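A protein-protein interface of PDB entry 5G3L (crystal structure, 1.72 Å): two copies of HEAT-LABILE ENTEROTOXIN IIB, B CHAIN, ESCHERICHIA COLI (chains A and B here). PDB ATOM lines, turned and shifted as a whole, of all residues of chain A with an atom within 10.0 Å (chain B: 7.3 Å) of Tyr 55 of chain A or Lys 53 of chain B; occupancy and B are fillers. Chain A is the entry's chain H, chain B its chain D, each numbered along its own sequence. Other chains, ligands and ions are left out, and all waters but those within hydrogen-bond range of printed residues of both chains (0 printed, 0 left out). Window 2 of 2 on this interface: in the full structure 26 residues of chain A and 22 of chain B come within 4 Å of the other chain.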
ATOM      1  N   ARG A  51     -28.275  16.829   1.218  1.00  0.00           N
ATOM      2  CA  ARG A  51     -27.692  17.009  -0.094  1.00  0.00           C
ATOM      3  C   ARG A  51     -26.370  17.822  -0.032  1.00  0.00           C
ATOM      4  O   ARG A  51     -26.110  18.552   0.931  1.00  0.00           O
ATOM      5  CB  ARG A  51     -28.654  17.693  -1.007  1.00  0.00           C
ATOM      6  CG  ARG A  51     -29.092  19.063  -0.498  1.00  0.00           C
ATOM      7  CD  ARG A  51     -29.844  19.648  -1.660  1.00  0.00           C
ATOM      8  NE  ARG A  51     -30.582  20.857  -1.304  1.00  0.00           N
ATOM      9  CZ  ARG A  51     -30.087  22.070  -1.252  1.00  0.00           C
ATOM     10  NH1 ARG A  51     -28.814  22.304  -1.509  1.00  0.00           N
ATOM     11  NH2 ARG A  51     -30.871  23.071  -0.943  1.00  0.00           N
ATOM     12  N   ALA A  52     -25.584  17.693  -1.071  1.00  0.00           N
ATOM     13  CA  ALA A  52     -24.223  18.326  -1.147  1.00  0.00           C
ATOM     14  C   ALA A  52     -23.779  18.407  -2.583  1.00  0.00           C
ATOM     15  O   ALA A  52     -23.918  17.439  -3.315  1.00  0.00           O
ATOM     16  CB  ALA A  52     -23.228  17.521  -0.357  1.00  0.00           C
ATOM     17  N   LYS A  53     -23.282  19.569  -2.997  1.00  0.00           N
ATOM     18  CA  LYS A  53     -22.874  19.727  -4.387  1.00  0.00           C
ATOM     19  C   LYS A  53     -21.540  19.031  -4.727  1.00  0.00           C
ATOM     20  O   LYS A  53     -21.376  18.514  -5.817  1.00  0.00           O
ATOM     21  CB  LYS A  53     -22.774  21.196  -4.750  1.00  0.00           C
ATOM     22  CG  LYS A  53     -22.530  21.491  -6.207  1.00  0.00           C
ATOM     23  CD  LYS A  53     -22.640  22.969  -6.454  1.00  0.00           C
ATOM     24  CE  LYS A  53     -22.575  23.323  -7.927  1.00  0.00           C
ATOM     25  N   ASP A  54     -20.612  19.069  -3.802  1.00  0.00           N
ATOM     26  CA  ASP A  54     -19.227  18.682  -4.121  1.00  0.00           C
ATOM     27  C   ASP A  54     -18.769  17.440  -3.459  1.00  0.00           C
ATOM     28  O   ASP A  54     -19.375  16.970  -2.499  1.00  0.00           O
ATOM     29  CB  ASP A  54     -18.260  19.823  -3.722  1.00  0.00           C
ATOM     30  CG  ASP A  54     -18.570  21.112  -4.439  1.00  0.00           C
ATOM     31  OD1 ASP A  54     -18.924  21.049  -5.645  1.00  0.00           O
ATOM     32  OD2 ASP A  54     -18.470  22.159  -3.783  1.00  0.00           O
ATOM     33  N   TYR A  55     -17.608  16.976  -3.935  1.00  0.00           N
ATOM     34  CA  TYR A  55     -16.952  15.799  -3.401  1.00  0.00           C
ATOM     35  C   TYR A  55     -16.337  16.117  -2.063  1.00  0.00           C
ATOM     36  O   TYR A  55     -15.813  17.221  -1.907  1.00  0.00           O
ATOM     37  CB  TYR A  55     -15.954  15.326  -4.450  1.00  0.00           C
ATOM     38  CG  TYR A  55     -15.136  14.147  -4.021  1.00  0.00           C
ATOM     39  CD1 TYR A  55     -13.971  14.322  -3.261  1.00  0.00           C
ATOM     40  CD2 TYR A  55     -15.493  12.866  -4.385  1.00  0.00           C
ATOM     41  CE1 TYR A  55     -13.214  13.228  -2.856  1.00  0.00           C
ATOM     42  CE2 TYR A  55     -14.738  11.778  -4.020  1.00  0.00           C
ATOM     43  CZ  TYR A  55     -13.604  11.953  -3.252  1.00  0.00           C
ATOM     44  OH  TYR A  55     -12.899  10.867  -2.836  1.00  0.00           O
ATOM     45  N   PRO A  56     -16.392  15.244  -1.065  1.00  0.00           N
ATOM     46  CA  PRO A  56     -16.902  13.847  -1.175  1.00  0.00           C
ATOM     47  C   PRO A  56     -18.369  13.632  -0.745  1.00  0.00           C
ATOM     48  O   PRO A  56     -18.915  12.548  -0.959  1.00  0.00           O
ATOM     49  CB  PRO A  56     -16.043  13.113  -0.177  1.00  0.00           C
ATOM     50  CG  PRO A  56     -15.810  14.124   0.912  1.00  0.00           C
ATOM     51  CD  PRO A  56     -15.620  15.415   0.189  1.00  0.00           C
ATOM     52  N   ASP A  57     -19.018  14.657  -0.205  1.00  0.00           N
ATOM     53  CA  ASP A  57     -20.362  14.453   0.340  1.00  0.00           C
ATOM     54  C   ASP A  57     -21.369  14.222  -0.779  1.00  0.00           C
ATOM     55  O   ASP A  57     -22.468  13.688  -0.526  1.00  0.00           O
ATOM     56  CB  ASP A  57     -20.829  15.568   1.279  1.00  0.00           C
ATOM     57  CG  ASP A  57     -20.152  15.505   2.644  1.00  0.00           C
ATOM     58  OD1 ASP A  57     -19.514  14.504   2.963  1.00  0.00           O
ATOM     59  OD2 ASP A  57     -20.261  16.484   3.399  1.00  0.00           O
ATOM     60  N   ASN A  58     -21.075  14.669  -1.990  1.00  0.00           N
ATOM     61  CA  ASN A  58     -21.980  14.368  -3.098  1.00  0.00           C
ATOM     62  C   ASN A  58     -22.111  12.860  -3.357  1.00  0.00           C
ATOM     63  O   ASN A  58     -23.189  12.388  -3.786  1.00  0.00           O
ATOM     64  CB  ASN A  58     -21.659  15.147  -4.361  1.00  0.00           C
ATOM     65  CG  ASN A  58     -20.336  14.774  -4.963  1.00  0.00           C
ATOM     66  OD1 ASN A  58     -19.548  13.998  -4.418  1.00  0.00           O
ATOM     67  ND2 ASN A  58     -20.066  15.384  -6.085  1.00  0.00           N
ATOM     68  N   VAL A  59     -21.082  12.095  -3.038  1.00  0.00           N
ATOM     69  CA  VAL A  59     -21.171  10.599  -3.104  1.00  0.00           C
ATOM     70  C   VAL A  59     -22.102  10.040  -2.042  1.00  0.00           C
ATOM     71  O   VAL A  59     -23.085   9.317  -2.359  1.00  0.00           O
ATOM     72  CB  VAL A  59     -19.761   9.958  -2.941  1.00  0.00           C
ATOM     73  CG1 VAL A  59     -19.852   8.449  -2.805  1.00  0.00           C
ATOM     74  CG2 VAL A  59     -18.904  10.379  -4.151  1.00  0.00           C
ATOM     75  N   MET A  60     -21.827  10.367  -0.788  1.00  0.00           N
ATOM     76  CA  MET A  60     -22.635   9.812   0.287  1.00  0.00           C
ATOM     77  C   MET A  60     -24.126  10.201   0.108  1.00  0.00           C
ATOM     78  O   MET A  60     -25.016   9.380   0.405  1.00  0.00           O
ATOM     79  CB  MET A  60     -22.109  10.243   1.670  1.00  0.00           C
ATOM     80  CG  MET A  60     -21.024   9.381   2.205  1.00  0.00           C
ATOM     81  SD  MET A  60     -19.411   9.627   1.412  1.00  0.00           S
ATOM     82  CE  MET A  60     -18.872  11.095   2.183  1.00  0.00           C
ATOM     83  N   THR A  61     -24.390  11.457  -0.236  1.00  0.00           N
ATOM     84  CA  THR A  61     -25.793  11.918  -0.331  1.00  0.00           C
ATOM     85  C   THR A  61     -26.524  11.205  -1.502  1.00  0.00           C
ATOM     86  O   THR A  61     -27.663  10.780  -1.370  1.00  0.00           O
ATOM     87  CB  THR A  61     -25.930  13.456  -0.439  1.00  0.00           C
ATOM     88  OG1 THR A  61     -25.195  13.926  -1.560  1.00  0.00           O
ATOM     89  CG2 THR A  61     -25.481  14.111   0.854  1.00  0.00           C
ATOM     90  N   SER B  50     -13.594   2.148  -0.704  1.00  0.00           N
ATOM     91  CA  SER B  50     -12.752   3.188  -1.228  1.00  0.00           C
ATOM     92  C   SER B  50     -13.524   4.347  -1.898  1.00  0.00           C
ATOM     93  O   SER B  50     -14.559   4.129  -2.511  1.00  0.00           O
ATOM     94  CB  SER B  50     -11.720   2.582  -2.228  1.00  0.00           C
ATOM     95  OG  SER B  50     -10.758   1.692  -1.610  1.00  0.00           O
ATOM     96  N   ARG B  51     -13.002   5.561  -1.802  1.00  0.00           N
ATOM     97  CA  ARG B  51     -13.510   6.651  -2.635  1.00  0.00           C
ATOM     98  C   ARG B  51     -12.388   7.351  -3.439  1.00  0.00           C
ATOM     99  O   ARG B  51     -11.228   7.300  -3.063  1.00  0.00           O
ATOM    100  CB  ARG B  51     -14.290   7.677  -1.794  1.00  0.00           C
ATOM    101  CG  ARG B  51     -13.397   8.423  -0.809  1.00  0.00           C
ATOM    102  CD  ARG B  51     -13.902   9.821  -0.445  1.00  0.00           C
ATOM    103  NE  ARG B  51     -14.747   9.730   0.690  1.00  0.00           N
ATOM    104  CZ  ARG B  51     -14.621  10.393   1.826  1.00  0.00           C
ATOM    105  NH1 ARG B  51     -13.662  11.306   2.050  1.00  0.00           N
ATOM    106  NH2 ARG B  51     -15.495  10.118   2.761  1.00  0.00           N
ATOM    107  N   ALA B  52     -12.789   8.007  -4.507  1.00  0.00           N
ATOM    108  CA  ALA B  52     -11.904   8.724  -5.380  1.00  0.00           C
ATOM    109  C   ALA B  52     -12.654   9.754  -6.174  1.00  0.00           C
ATOM    110  O   ALA B  52     -13.660   9.466  -6.775  1.00  0.00           O
ATOM    111  CB  ALA B  52     -11.212   7.745  -6.333  1.00  0.00           C
ATOM    112  N   LYS B  53     -12.108  10.968  -6.233  1.00  0.00           N
ATOM    113  CA  LYS B  53     -12.754  12.063  -6.971  1.00  0.00           C
ATOM    114  C   LYS B  53     -12.589  11.972  -8.491  1.00  0.00           C
ATOM    115  O   LYS B  53     -13.491  12.290  -9.245  1.00  0.00           O
ATOM    116  CB  LYS B  53     -12.240  13.424  -6.494  1.00  0.00           C
ATOM    117  CG  LYS B  53     -12.959  14.628  -7.102  1.00  0.00           C
ATOM    118  CD  LYS B  53     -12.520  15.967  -6.461  1.00  0.00           C
ATOM    119  CE  LYS B  53     -11.155  16.427  -6.937  1.00  0.00           C
ATOM    120  NZ  LYS B  53     -11.172  16.869  -8.362  1.00  0.00           N
ATOM    121  N   ASP B  54     -11.428  11.527  -8.931  1.00  0.00           N
ATOM    122  CA  ASP B  54     -11.063  11.627 -10.351  1.00  0.00           C
ATOM    123  C   ASP B  54     -10.925  10.320 -11.074  1.00  0.00           C
ATOM    124  O   ASP B  54     -10.861   9.274 -10.468  1.00  0.00           O
ATOM    125  CB  ASP B  54      -9.722  12.362 -10.458  1.00  0.00           C
ATOM    126  CG  ASP B  54      -9.767  13.752  -9.859  1.00  0.00           C
ATOM    127  OD1 ASP B  54     -10.775  14.437 -10.036  1.00  0.00           O
ATOM    128  OD2 ASP B  54      -8.765  14.142  -9.242  1.00  0.00           O
ATOM    129  N   TYR B  55     -10.923  10.453 -12.379  1.00  0.00           N
ATOM    130  CA  TYR B  55     -10.789   9.358 -13.295  1.00  0.00           C
ATOM    131  C   TYR B  55      -9.364   8.808 -13.198  1.00  0.00           C
ATOM    132  O   TYR B  55      -8.435   9.614 -13.087  1.00  0.00           O
ATOM    133  CB  TYR B  55     -11.152   9.842 -14.706  1.00  0.00           C
ATOM    134  CG  TYR B  55     -10.948   8.814 -15.779  1.00  0.00           C
ATOM    135  CD1 TYR B  55      -9.699   8.637 -16.374  1.00  0.00           C
ATOM    136  CD2 TYR B  55     -11.992   8.032 -16.207  1.00  0.00           C
ATOM    137  CE1 TYR B  55      -9.509   7.716 -17.369  1.00  0.00           C
ATOM    138  CE2 TYR B  55     -11.811   7.110 -17.215  1.00  0.00           C
ATOM    139  CZ  TYR B  55     -10.588   6.936 -17.770  1.00  0.00           C
ATOM    140  OH  TYR B  55     -10.415   6.017 -18.760  1.00  0.00           O
ATOM    141  N   ASP B  57     -10.303   6.121 -11.110  1.00  0.00           N
ATOM    142  CA  ASP B  57     -10.765   5.410  -9.878  1.00  0.00           C
ATOM    143  C   ASP B  57     -12.131   5.844  -9.462  1.00  0.00           C
ATOM    144  O   ASP B  57     -12.799   5.122  -8.733  1.00  0.00           O
ATOM    145  CB  ASP B  57      -9.775   5.554  -8.709  1.00  0.00           C
ATOM    146  CG  ASP B  57      -8.547   4.644  -8.854  1.00  0.00           C
ATOM    147  OD1 ASP B  57      -8.485   3.825  -9.740  1.00  0.00           O
ATOM    148  OD2 ASP B  57      -7.599   4.779  -8.090  1.00  0.00           O
ATOM    149  N   ASN B  58     -12.569   6.999  -9.921  1.00  0.00           N
ATOM    150  CA  ASN B  58     -13.987   7.383  -9.664  1.00  0.00           C
ATOM    151  C   ASN B  58     -14.981   6.388 -10.263  1.00  0.00           C
ATOM    152  O   ASN B  58     -16.061   6.163  -9.719  1.00  0.00           O
ATOM    153  CB  ASN B  58     -14.311   8.831 -10.041  1.00  0.00           C
ATOM    154  CG  ASN B  58     -14.190   9.115 -11.501  1.00  0.00           C
ATOM    155  OD1 ASN B  58     -13.745   8.295 -12.309  1.00  0.00           O
ATOM    156  ND2 ASN B  58     -14.516  10.343 -11.849  1.00  0.00           N
ATOM    157  N   VAL B  59     -14.617   5.782 -11.376  1.00  0.00           N
ATOM    158  CA  VAL B  59     -15.417   4.720 -11.992  1.00  0.00           C
ATOM    159  C   VAL B  59     -15.442   3.474 -11.126  1.00  0.00           C
ATOM    160  O   VAL B  59     -16.499   2.937 -10.758  1.00  0.00           O
ATOM    161  CB  VAL B  59     -14.901   4.380 -13.413  1.00  0.00           C
ATOM    162  CG1 VAL B  59     -15.591   3.143 -13.954  1.00  0.00           C
ATOM    163  CG2 VAL B  59     -15.106   5.584 -14.320  1.00  0.00           C
ATOM    164  N   THR B  61     -14.668   2.946  -8.026  1.00  0.00           N
ATOM    165  CA  THR B  61     -15.270   3.126  -6.665  1.00  0.00           C
ATOM    166  C   THR B  61     -16.802   3.248  -6.755  1.00  0.00           C
ATOM    167  O   THR B  61     -17.514   2.657  -5.949  1.00  0.00           O
ATOM    168  CB  THR B  61     -14.705   4.332  -5.886  1.00  0.00           C
ATOM    169  OG1 THR B  61     -14.845   5.548  -6.643  1.00  0.00           O
ATOM    170  CG2 THR B  61     -13.210   4.097  -5.550  1.00  0.00           C
ATOM    171  N   ARG B  65     -19.590   0.575  -4.970  1.00  0.00           N
ATOM    172  CA  ARG B  65     -20.873   0.934  -4.327  1.00  0.00           C
ATOM    173  C   ARG B  65     -22.051   0.166  -4.932  1.00  0.00           C
ATOM    174  O   ARG B  65     -22.966  -0.265  -4.230  1.00  0.00           O
ATOM    175  CB  ARG B  65     -21.075   2.460  -4.323  1.00  0.00           C
ATOM    176  CG  ARG B  65     -20.038   3.214  -3.514  1.00  0.00           C
ATOM    177  CD  ARG B  65     -20.360   4.650  -3.373  1.00  0.00           C
ATOM    178  NE  ARG B  65     -20.467   5.399  -4.600  1.00  0.00           N
ATOM    179  CZ  ARG B  65     -19.421   5.986  -5.200  1.00  0.00           C
ATOM    180  NH1 ARG B  65     -18.203   5.928  -4.678  1.00  0.00           N
ATOM    181  NH2 ARG B  65     -19.625   6.694  -6.292  1.00  0.00           N
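Of the 11 printed residues of chain B, 4 touch a printed residue of chain A.
Along chain B the printed residues that touch a printed residue of chain A span positions 51 to 65.
Of the 11 printed residues of chain A, 4 touch a printed residue of chain B.
Among the printed residues, 6 pairs touch across the chains.
Among the printed residues, no Asp or Glu carboxylate lies within 4 Å of a Lys or Arg side-chain nitrogen of the other chain.
Tyr 55 of chain A touches Arg 51 of chain B, but with the chains exchanged Arg 51 of chain A does not touch Tyr 55 of chain B (21.1 Å).
Tyr 55 of chain A touches Ala 52 of chain B, but with the chains exchanged Ala 52 of chain A does not touch Tyr 55 of chain B (17.3 Å).
Tyr 55 of chain A touches Lys 53 of chain B, but with the chains exchanged Lys 53 of chain A does not touch Tyr 55 of chain B (14.7 Å).
Positions printed for both chains: 51, 52, 53, 54, 55, 57, 58, 59 and 61.
NZ of Lys 53 of chain B lies within salt-bridge range of OD1 of Asp 54 of chain B (3.0 Å).
The backbone carbonyl oxygen (O) of Lys 53 of chain B sits at hydrogen-bond distance from the side-chain amide nitrogen (ND2) of Asn 58 of chain B (3.4 Å).
Of the printed residues of chain B, Tyr 55 of chain A touches Arg 51, Ala 52 and Lys 53.
Of the printed residues of chain A, Lys 53 of chain B touches Tyr 55 (3.5 Å).
Ala 52 of chain B touches just one residue of chain A: Tyr 55.
No residue of chain A comes within 4 Å of Asp 54 of chain B.
Printed residues of chain A within 4 Å of Arg 65 of chain B: Val 59 (3.5 Å).
Of the printed residues of chain B, Val 59 of chain A touches Arg 65.
Thr 61 of chain A touches none of the printed residues of chain B.
Val 59 of chain B touches none of the printed residues of chain A.
The nearest printed residue of chain B that does not touch Tyr 55 of chain A is Asp 54 of chain B (5.9 Å).
N of Ala 52 of chain B lies within hydrogen-bond range of OH of Tyr 55 of chain A (3.3 Å).
N of Lys 53 of chain B lies close to OH of Tyr 55 of chain A (3.5 Å).
CD of Arg 51 of chain B touches OH of Tyr 55 of chain A, 2.8 Å away.
Pro 56 of chain A touches Arg 51 of chain B (CB to CZ, 3.7 Å).
Arg 65 of chain B touches Val 59 of chain A.
Met 60 of chain A touches Arg 51 of chain B.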
